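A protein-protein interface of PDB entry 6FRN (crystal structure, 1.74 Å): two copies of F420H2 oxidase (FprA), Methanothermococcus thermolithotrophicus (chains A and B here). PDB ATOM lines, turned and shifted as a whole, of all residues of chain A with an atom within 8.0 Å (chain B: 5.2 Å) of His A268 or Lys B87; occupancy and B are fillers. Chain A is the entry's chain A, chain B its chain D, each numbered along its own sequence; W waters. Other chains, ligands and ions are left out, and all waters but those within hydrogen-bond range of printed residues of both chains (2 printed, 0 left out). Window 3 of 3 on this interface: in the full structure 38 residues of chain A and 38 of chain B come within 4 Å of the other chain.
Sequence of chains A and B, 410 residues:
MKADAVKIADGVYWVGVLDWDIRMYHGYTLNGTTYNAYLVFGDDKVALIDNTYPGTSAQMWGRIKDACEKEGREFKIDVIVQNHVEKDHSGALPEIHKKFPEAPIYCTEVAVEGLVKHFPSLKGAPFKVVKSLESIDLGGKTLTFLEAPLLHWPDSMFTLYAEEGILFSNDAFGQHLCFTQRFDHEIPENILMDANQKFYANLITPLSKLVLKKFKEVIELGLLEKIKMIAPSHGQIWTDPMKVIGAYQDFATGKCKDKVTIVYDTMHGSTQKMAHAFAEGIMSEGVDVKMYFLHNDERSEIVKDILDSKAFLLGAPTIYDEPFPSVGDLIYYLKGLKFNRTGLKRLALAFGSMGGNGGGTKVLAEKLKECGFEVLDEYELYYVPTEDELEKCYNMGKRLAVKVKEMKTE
CE1 of His A268 touches OH of Tyr B25 (3.4 Å).
Val B85 touches Tyr A383.
CE1 of His B118 touches CG of Tyr A383 (3.4 Å).
Val A384 touches His B118 (CG2 to CD2, 3.9 Å).
No position is printed for both chains.
Of the 14 printed residues of chain A, 3 touch a printed residue of chain B.
Printed residues of chain A that touch a printed residue of chain B: His A268, Tyr A383 and Val A384.
Printed residues of chain B that touch a printed residue of chain A: Tyr B25, Val B85, Lys B87 and His B118.
Among the printed residues, no Asp or Glu carboxylate lies within 4 Å of a Lys or Arg side-chain nitrogen of the other chain.
The backbone carbonyl oxygen of His A268 lies within hydrogen-bond range of the side-chain amino group of Lys B87 (3.0 Å).
Water W2 lies within hydrogen-bond range of a ring nitrogen (ND1) of His A268 (2.7 Å), the side-chain hydroxyl of Tyr B53 (2.8 Å) and the backbone carbonyl oxygen of Met A267 (2.9 Å).
Water W1 bridges OE1 of Glu B86 and NE2 of His A268.
The side-chain hydroxyl (OG) of Ser A270 lies within hydrogen-bond range of the backbone carbonyl oxygen (O) of Tyr A383, at 3.3 Å.
The side-chain hydroxyl (OG) of Ser A353 is in hydrogen-bond range of the backbone carbonyl oxygen (O) of Tyr A383 (2.7 Å).
OD1 of Asp B88 sits close to OH of Tyr B25 (3.2 Å).
The backbone carbonyl oxygen of Val B85 sits at hydrogen-bond distance from the side-chain hydroxyl of Ser B90 (2.8 Å).
Of the printed residues of chain B, Tyr A383 touches Val B85 (2.9 Å) and His B118 (3.4 Å).
Of the printed residues of chain A, Tyr B25 touches His A268.
Tyr B53 touches none of the printed residues of chain A.
Of the printed residues of chain A, Val B85 touches Tyr A383.
Lys B87 touches just one residue of chain A: His A268 (3.0 Å).
Printed residues of chain A within 4 Å of His B118: Tyr A383 and Val A384.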
ATOM      1  N   ASP A 265     -26.367 -22.775  -7.056  1.00  0.00           N
ATOM      2  CA  ASP A 265     -26.301 -21.368  -6.673  1.00  0.00           C
ATOM      3  C   ASP A 265     -25.504 -21.278  -5.372  1.00  0.00           C
ATOM      4  O   ASP A 265     -25.314 -22.283  -4.708  1.00  0.00           O
ATOM      5  CB  ASP A 265     -27.644 -20.633  -6.569  1.00  0.00           C
ATOM      6  CG  ASP A 265     -27.569 -19.148  -6.981  1.00  0.00           C
ATOM      7  OD1 ASP A 265     -26.464 -18.554  -6.911  1.00  0.00           O
ATOM      8  OD2 ASP A 265     -28.614 -18.593  -7.396  1.00  0.00           O
ATOM      9  N   THR A 266     -24.993 -20.086  -5.051  1.00  0.00           N
ATOM     10  CA  THR A 266     -24.157 -19.885  -3.862  1.00  0.00           C
ATOM     11  C   THR A 266     -24.261 -18.434  -3.421  1.00  0.00           C
ATOM     12  O   THR A 266     -24.500 -17.558  -4.248  1.00  0.00           O
ATOM     13  CB  THR A 266     -22.686 -20.269  -4.172  1.00  0.00           C
ATOM     14  OG1 THR A 266     -21.954 -20.426  -2.956  1.00  0.00           O
ATOM     15  CG2 THR A 266     -21.964 -19.239  -5.028  1.00  0.00           C
ATOM     16  N   MET A 267     -24.129 -18.198  -2.140  1.00  0.00           N
ATOM     17  CA  MET A 267     -24.089 -16.872  -1.538  1.00  0.00           C
ATOM     18  C   MET A 267     -22.641 -16.471  -1.199  1.00  0.00           C
ATOM     19  O   MET A 267     -22.228 -15.336  -1.488  1.00  0.00           O
ATOM     20  CB  MET A 267     -24.967 -16.809  -0.295  1.00  0.00           C
ATOM     21  CG  MET A 267     -26.410 -17.159  -0.573  1.00  0.00           C
ATOM     22  SD  MET A 267     -27.471 -17.031   0.880  1.00  0.00           S
ATOM     23  CE  MET A 267     -26.923 -18.433   1.837  1.00  0.00           C
ATOM     24  N   HIS A 268     -21.901 -17.384  -0.550  1.00  0.00           N
ATOM     25  CA  HIS A 268     -20.509 -17.172  -0.107  1.00  0.00           C
ATOM     26  C   HIS A 268     -19.458 -18.029  -0.832  1.00  0.00           C
ATOM     27  O   HIS A 268     -18.275 -17.906  -0.514  1.00  0.00           O
ATOM     28  CB  HIS A 268     -20.394 -17.399   1.396  1.00  0.00           C
ATOM     29  CG  HIS A 268     -21.238 -16.516   2.264  1.00  0.00           C
ATOM     30  ND1 HIS A 268     -21.128 -15.139   2.221  1.00  0.00           N
ATOM     31  CD2 HIS A 268     -22.105 -16.853   3.253  1.00  0.00           C
ATOM     32  CE1 HIS A 268     -21.895 -14.676   3.197  1.00  0.00           C
ATOM     33  NE2 HIS A 268     -22.551 -15.661   3.815  1.00  0.00           N
ATOM     34  N   GLY A 269     -19.864 -18.901  -1.746  1.00  0.00           N
ATOM     35  CA  GLY A 269     -18.948 -19.726  -2.531  1.00  0.00           C
ATOM     36  C   GLY A 269     -18.741 -21.179  -2.136  1.00  0.00           C
ATOM     37  O   GLY A 269     -18.136 -21.937  -2.906  1.00  0.00           O
ATOM     38  N   SER A 270     -19.260 -21.619  -0.997  1.00  0.00           N
ATOM     39  CA  SER A 270     -19.039 -23.013  -0.551  1.00  0.00           C
ATOM     40  C   SER A 270     -19.721 -24.058  -1.430  1.00  0.00           C
ATOM     41  O   SER A 270     -19.088 -25.059  -1.804  1.00  0.00           O
ATOM     42  CB  SER A 270     -19.418 -23.174   0.906  1.00  0.00           C
ATOM     43  OG  SER A 270     -18.481 -22.406   1.650  1.00  0.00           O
ATOM     44  N   THR A 271     -20.980 -23.808  -1.836  1.00  0.00           N
ATOM     45  CA  THR A 271     -21.682 -24.724  -2.731  1.00  0.00           C
ATOM     46  C   THR A 271     -21.002 -24.792  -4.060  1.00  0.00           C
ATOM     47  O   THR A 271     -20.970 -25.865  -4.669  1.00  0.00           O
ATOM     48  CB  THR A 271     -23.166 -24.365  -2.810  1.00  0.00           C
ATOM     49  OG1 THR A 271     -23.697 -24.413  -1.487  1.00  0.00           O
ATOM     50  CG2 THR A 271     -23.941 -25.321  -3.668  1.00  0.00           C
ATOM     51  N   GLN A 272     -20.411 -23.666  -4.518  1.00  0.00           N
ATOM     52  CA  GLN A 272     -19.636 -23.648  -5.758  1.00  0.00           C
ATOM     53  C   GLN A 272     -18.446 -24.598  -5.661  1.00  0.00           C
ATOM     54  O   GLN A 272     -18.190 -25.380  -6.574  1.00  0.00           O
ATOM     55  CB  GLN A 272     -19.144 -22.226  -6.041  1.00  0.00           C
ATOM     56  CG  GLN A 272     -18.267 -22.111  -7.250  1.00  0.00           C
ATOM     57  CD  GLN A 272     -17.920 -20.666  -7.462  1.00  0.00           C
ATOM     58  OE1 GLN A 272     -16.964 -20.177  -6.874  1.00  0.00           O
ATOM     59  NE2 GLN A 272     -18.791 -19.903  -8.113  1.00  0.00           N
ATOM     60  N   LYS A 273     -17.692 -24.517  -4.563  1.00  0.00           N
ATOM     61  CA  LYS A 273     -16.558 -25.431  -4.339  1.00  0.00           C
ATOM     62  C   LYS A 273     -16.991 -26.891  -4.384  1.00  0.00           C
ATOM     63  O   LYS A 273     -16.340 -27.691  -5.047  1.00  0.00           O
ATOM     64  CB  LYS A 273     -15.862 -25.150  -3.020  1.00  0.00           C
ATOM     65  CG  LYS A 273     -15.153 -23.825  -2.982  1.00  0.00           C
ATOM     66  CD  LYS A 273     -14.647 -23.549  -1.584  1.00  0.00           C
ATOM     67  CE  LYS A 273     -13.844 -22.274  -1.479  1.00  0.00           C
ATOM     68  NZ  LYS A 273     -14.701 -21.058  -1.429  1.00  0.00           N
ATOM     69  N   PRO A 317     -27.173 -23.532  -1.139  1.00  0.00           N
ATOM     70  CA  PRO A 317     -27.107 -23.387   0.313  1.00  0.00           C
ATOM     71  C   PRO A 317     -28.486 -23.214   0.935  1.00  0.00           C
ATOM     72  O   PRO A 317     -29.462 -22.900   0.233  1.00  0.00           O
ATOM     73  CB  PRO A 317     -26.288 -22.122   0.469  1.00  0.00           C
ATOM     74  CG  PRO A 317     -26.705 -21.284  -0.663  1.00  0.00           C
ATOM     75  CD  PRO A 317     -26.790 -22.272  -1.810  1.00  0.00           C
ATOM     76  N   PHE A 324     -31.630 -21.977  -1.517  1.00  0.00           N
ATOM     77  CA  PHE A 324     -31.529 -20.649  -2.143  1.00  0.00           C
ATOM     78  C   PHE A 324     -32.624 -20.496  -3.204  1.00  0.00           C
ATOM     79  O   PHE A 324     -32.790 -21.411  -4.012  1.00  0.00           O
ATOM     80  CB  PHE A 324     -30.123 -20.380  -2.663  1.00  0.00           C
ATOM     81  CG  PHE A 324     -29.941 -18.926  -2.987  1.00  0.00           C
ATOM     82  CD1 PHE A 324     -29.696 -18.000  -1.979  1.00  0.00           C
ATOM     83  CD2 PHE A 324     -30.217 -18.448  -4.253  1.00  0.00           C
ATOM     84  CE1 PHE A 324     -29.661 -16.641  -2.258  1.00  0.00           C
ATOM     85  CE2 PHE A 324     -30.141 -17.091  -4.539  1.00  0.00           C
ATOM     86  CZ  PHE A 324     -29.901 -16.195  -3.537  1.00  0.00           C
ATOM     87  N   SER A 353     -24.327 -26.290   1.175  1.00  0.00           N
ATOM     88  CA  SER A 353     -23.682 -25.885   2.417  1.00  0.00           C
ATOM     89  C   SER A 353     -24.726 -25.215   3.307  1.00  0.00           C
ATOM     90  O   SER A 353     -25.716 -24.686   2.808  1.00  0.00           O
ATOM     91  CB  SER A 353     -22.509 -24.953   2.111  1.00  0.00           C
ATOM     92  OG  SER A 353     -21.897 -24.493   3.309  1.00  0.00           O
ATOM     93  N   TYR A 383     -20.677 -24.743   6.405  1.00  0.00           N
ATOM     94  CA  TYR A 383     -19.821 -23.645   5.906  1.00  0.00           C
ATOM     95  C   TYR A 383     -18.807 -24.100   4.835  1.00  0.00           C
ATOM     96  O   TYR A 383     -19.215 -24.746   3.852  1.00  0.00           O
ATOM     97  CB  TYR A 383     -19.137 -22.884   7.065  1.00  0.00           C
ATOM     98  CG  TYR A 383     -20.073 -22.114   7.969  1.00  0.00           C
ATOM     99  CD1 TYR A 383     -21.063 -21.289   7.444  1.00  0.00           C
ATOM    100  CD2 TYR A 383     -19.873 -22.085   9.342  1.00  0.00           C
ATOM    101  CE1 TYR A 383     -21.854 -20.492   8.271  1.00  0.00           C
ATOM    102  CE2 TYR A 383     -20.657 -21.291  10.173  1.00  0.00           C
ATOM    103  CZ  TYR A 383     -21.675 -20.529   9.635  1.00  0.00           C
ATOM    104  OH  TYR A 383     -22.476 -19.758  10.450  1.00  0.00           O
ATOM    105  N   VAL A 384     -17.511 -23.760   4.977  1.00  0.00           N
ATOM    106  CA  VAL A 384     -16.523 -24.002   3.935  1.00  0.00           C
ATOM    107  C   VAL A 384     -16.095 -25.456   3.968  1.00  0.00           C
ATOM    108  O   VAL A 384     -15.644 -25.924   5.015  1.00  0.00           O
ATOM    109  CB  VAL A 384     -15.310 -23.049   4.108  1.00  0.00           C
ATOM    110  CG1 VAL A 384     -14.290 -23.251   3.004  1.00  0.00           C
ATOM    111  CG2 VAL A 384     -15.760 -21.588   4.163  1.00  0.00           C
ATOM    112  N   TYR B  25     -25.932  -8.975  -2.802  1.00  0.00           N
ATOM    113  CA  TYR B  25     -25.342  -9.796  -1.751  1.00  0.00           C
ATOM    114  C   TYR B  25     -26.398 -10.812  -1.327  1.00  0.00           C
ATOM    115  O   TYR B  25     -27.436 -10.416  -0.857  1.00  0.00           O
ATOM    116  CB  TYR B  25     -24.927  -8.894  -0.587  1.00  0.00           C
ATOM    117  CG  TYR B  25     -24.357  -9.596   0.617  1.00  0.00           C
ATOM    118  CD1 TYR B  25     -23.633 -10.778   0.488  1.00  0.00           C
ATOM    119  CD2 TYR B  25     -24.466  -9.038   1.884  1.00  0.00           C
ATOM    120  CE1 TYR B  25     -23.104 -11.425   1.599  1.00  0.00           C
ATOM    121  CE2 TYR B  25     -23.924  -9.665   2.989  1.00  0.00           C
ATOM    122  CZ  TYR B  25     -23.259 -10.870   2.848  1.00  0.00           C
ATOM    123  OH  TYR B  25     -22.707 -11.506   3.936  1.00  0.00           O
ATOM    124  N   THR B  52     -14.328  -7.321   8.624  1.00  0.00           N
ATOM    125  CA  THR B  52     -14.842  -7.061   7.304  1.00  0.00           C
ATOM    126  C   THR B  52     -14.670  -8.278   6.410  1.00  0.00           C
ATOM    127  O   THR B  52     -13.996  -9.219   6.795  1.00  0.00           O
ATOM    128  CB  THR B  52     -14.092  -5.815   6.700  1.00  0.00           C
ATOM    129  OG1 THR B  52     -14.773  -5.315   5.532  1.00  0.00           O
ATOM    130  CG2 THR B  52     -12.622  -6.067   6.422  1.00  0.00           C
ATOM    131  N   TYR B  53     -15.249  -8.174   5.221  1.00  0.00           N
ATOM    132  CA  TYR B  53     -15.262  -9.209   4.170  1.00  0.00           C
ATOM    133  C   TYR B  53     -13.871  -9.574   3.678  1.00  0.00           C
ATOM    134  O   TYR B  53     -13.018  -8.684   3.561  1.00  0.00           O
ATOM    135  CB  TYR B  53     -16.168  -8.721   3.011  1.00  0.00           C
ATOM    136  CG  TYR B  53     -16.620  -9.822   2.098  1.00  0.00           C
ATOM    137  CD1 TYR B  53     -15.868 -10.187   0.993  1.00  0.00           C
ATOM    138  CD2 TYR B  53     -17.817 -10.501   2.327  1.00  0.00           C
ATOM    139  CE1 TYR B  53     -16.227 -11.274   0.210  1.00  0.00           C
ATOM    140  CE2 TYR B  53     -18.230 -11.534   1.497  1.00  0.00           C
ATOM    141  CZ  TYR B  53     -17.440 -11.906   0.426  1.00  0.00           C
ATOM    142  OH  TYR B  53     -17.832 -12.945  -0.385  1.00  0.00           O
ATOM    143  N   PRO B  54     -13.563 -10.854   3.338  1.00  0.00           N
ATOM    144  CA  PRO B  54     -12.197 -11.166   2.873  1.00  0.00           C
ATOM    145  C   PRO B  54     -11.778 -10.319   1.680  1.00  0.00           C
ATOM    146  O   PRO B  54     -12.578 -10.105   0.758  1.00  0.00           O
ATOM    147  CB  PRO B  54     -12.293 -12.643   2.487  1.00  0.00           C
ATOM    148  CG  PRO B  54     -13.378 -13.163   3.334  1.00  0.00           C
ATOM    149  CD  PRO B  54     -14.383 -12.078   3.425  1.00  0.00           C
ATOM    150  N   VAL B  85     -20.065 -15.113  12.999  1.00  0.00           N
ATOM    151  CA  VAL B  85     -19.105 -15.899  12.232  1.00  0.00           C
ATOM    152  C   VAL B  85     -19.100 -15.532  10.739  1.00  0.00           C
ATOM    153  O   VAL B  85     -18.113 -15.807  10.073  1.00  0.00           O
ATOM    154  CB  VAL B  85     -19.334 -17.424  12.351  1.00  0.00           C
ATOM    155  CG1 VAL B  85     -19.259 -17.885  13.783  1.00  0.00           C
ATOM    156  CG2 VAL B  85     -20.652 -17.864  11.717  1.00  0.00           C
ATOM    157  N   GLU B  86     -20.215 -15.081  10.192  1.00  0.00           N
ATOM    158  CA  GLU B  86     -20.317 -14.832   8.765  1.00  0.00           C
ATOM    159  C   GLU B  86     -19.178 -13.944   8.246  1.00  0.00           C
ATOM    160  O   GLU B  86     -18.739 -13.026   8.935  1.00  0.00           O
ATOM    161  CB  GLU B  86     -21.689 -14.301   8.373  1.00  0.00           C
ATOM    162  CG  GLU B  86     -22.086 -13.061   9.134  1.00  0.00           C
ATOM    163  CD  GLU B  86     -23.312 -12.437   8.524  1.00  0.00           C
ATOM    164  OE1 GLU B  86     -24.022 -13.124   7.746  1.00  0.00           O
ATOM    165  OE2 GLU B  86     -23.567 -11.258   8.845  1.00  0.00           O
ATOM    166  N   LYS B  87     -18.655 -14.293   7.100  1.00  0.00           N
ATOM    167  CA  LYS B  87     -17.433 -13.702   6.534  1.00  0.00           C
ATOM    168  C   LYS B  87     -17.490 -12.201   6.252  1.00  0.00           C
ATOM    169  O   LYS B  87     -16.433 -11.595   6.161  1.00  0.00           O
ATOM    170  CB  LYS B  87     -16.999 -14.465   5.267  1.00  0.00           C
ATOM    171  CG  LYS B  87     -17.884 -14.200   4.068  1.00  0.00           C
ATOM    172  CD  LYS B  87     -17.736 -15.248   2.962  1.00  0.00           C
ATOM    173  CE  LYS B  87     -16.453 -15.166   2.222  1.00  0.00           C
ATOM    174  NZ  LYS B  87     -16.436 -16.078   1.044  1.00  0.00           N
ATOM    175  N   ASP B  88     -18.686 -11.592   6.140  1.00  0.00           N
ATOM    176  CA  ASP B  88     -18.757 -10.147   5.970  1.00  0.00           C
ATOM    177  C   ASP B  88     -18.315  -9.411   7.223  1.00  0.00           C
ATOM    178  O   ASP B  88     -17.954  -8.250   7.111  1.00  0.00           O
ATOM    179  CB  ASP B  88     -20.140  -9.652   5.492  1.00  0.00           C
ATOM    180  CG  ASP B  88     -21.323 -10.104   6.284  1.00  0.00           C
ATOM    181  OD1 ASP B  88     -21.274 -11.217   6.827  1.00  0.00           O
ATOM    182  OD2 ASP B  88     -22.337  -9.401   6.260  1.00  0.00           O
ATOM    183  N   HIS B  89     -18.246 -10.104   8.402  1.00  0.00           N
ATOM    184  CA  HIS B  89     -17.792  -9.499   9.665  1.00  0.00           C
ATOM    185  C   HIS B  89     -16.571 -10.191  10.262  1.00  0.00           C
ATOM    186  O   HIS B  89     -16.057  -9.681  11.235  1.00  0.00           O
ATOM    187  CB  HIS B  89     -18.930  -9.498  10.678  1.00  0.00           C
ATOM    188  CG  HIS B  89     -20.177  -8.941  10.063  1.00  0.00           C
ATOM    189  ND1 HIS B  89     -20.186  -7.703   9.511  1.00  0.00           N
ATOM    190  CD2 HIS B  89     -21.396  -9.509   9.905  1.00  0.00           C
ATOM    191  CE1 HIS B  89     -21.387  -7.550   8.961  1.00  0.00           C
ATOM    192  NE2 HIS B  89     -22.153  -8.622   9.177  1.00  0.00           N
ATOM    193  N   SER B  90     -16.122 -11.328   9.711  1.00  0.00           N
ATOM    194  CA  SER B  90     -14.994 -12.096  10.270  1.00  0.00           C
ATOM    195  C   SER B  90     -13.918 -12.390   9.244  1.00  0.00           C
ATOM    196  O   SER B  90     -12.895 -12.956   9.620  1.00  0.00           O
ATOM    197  CB  SER B  90     -15.498 -13.443  10.766  1.00  0.00           C
ATOM    198  OG  SER B  90     -15.844 -14.254   9.654  1.00  0.00           O
ATOM    199  N   GLY B  91     -14.093 -11.917   8.016  1.00  0.00           N
ATOM    200  CA  GLY B  91     -13.183 -12.178   6.908  1.00  0.00           C
ATOM    201  C   GLY B  91     -11.746 -11.736   7.099  1.00  0.00           C
ATOM    202  O   GLY B  91     -10.840 -12.310   6.488  1.00  0.00           O
ATOM    203  N   HIS B 118     -14.245 -21.880   8.672  1.00  0.00           N
ATOM    204  CA  HIS B 118     -13.957 -20.887   7.621  1.00  0.00           C
ATOM    205  C   HIS B 118     -12.441 -20.693   7.476  1.00  0.00           C
ATOM    206  O   HIS B 118     -11.924 -20.657   6.362  1.00  0.00           O
ATOM    207  CB  HIS B 118     -14.562 -19.509   7.980  1.00  0.00           C
ATOM    208  CG  HIS B 118     -16.012 -19.323   7.657  1.00  0.00           C
ATOM    209  ND1 HIS B 118     -17.010 -19.721   8.531  1.00  0.00           N
ATOM    210  CD2 HIS B 118     -16.589 -18.689   6.608  1.00  0.00           C
ATOM    211  CE1 HIS B 118     -18.153 -19.352   7.977  1.00  0.00           C
ATOM    212  NE2 HIS B 118     -17.956 -18.739   6.815  1.00  0.00           N
ATOM    213  N   PHE B 119     -11.734 -20.536   8.600  1.00  0.00           N
ATOM    214  CA  PHE B 119     -10.323 -20.156   8.634  1.00  0.00           C
ATOM    215  C   PHE B 119      -9.513 -21.136   9.469  1.00  0.00           C
ATOM    216  O   PHE B 119      -9.283 -20.903  10.650  1.00  0.00           O
ATOM    217  CB  PHE B 119     -10.213 -18.716   9.202  1.00  0.00           C
ATOM    218  CG  PHE B 119     -11.233 -17.755   8.633  1.00  0.00           C
ATOM    219  CD1 PHE B 119     -11.234 -17.433   7.280  1.00  0.00           C
ATOM    220  CD2 PHE B 119     -12.185 -17.162   9.451  1.00  0.00           C
ATOM    221  CE1 PHE B 119     -12.191 -16.559   6.750  1.00  0.00           C
ATOM    222  CE2 PHE B 119     -13.148 -16.301   8.921  1.00  0.00           C
ATOM    223  CZ  PHE B 119     -13.159 -16.014   7.569  1.00  0.00           C
HETATM  224  O   HOH W   1     -24.020 -15.564   6.297  1.00  0.00           O
HETATM  225  O   HOH W   2     -20.474 -13.597   0.058  1.00  0.00           O
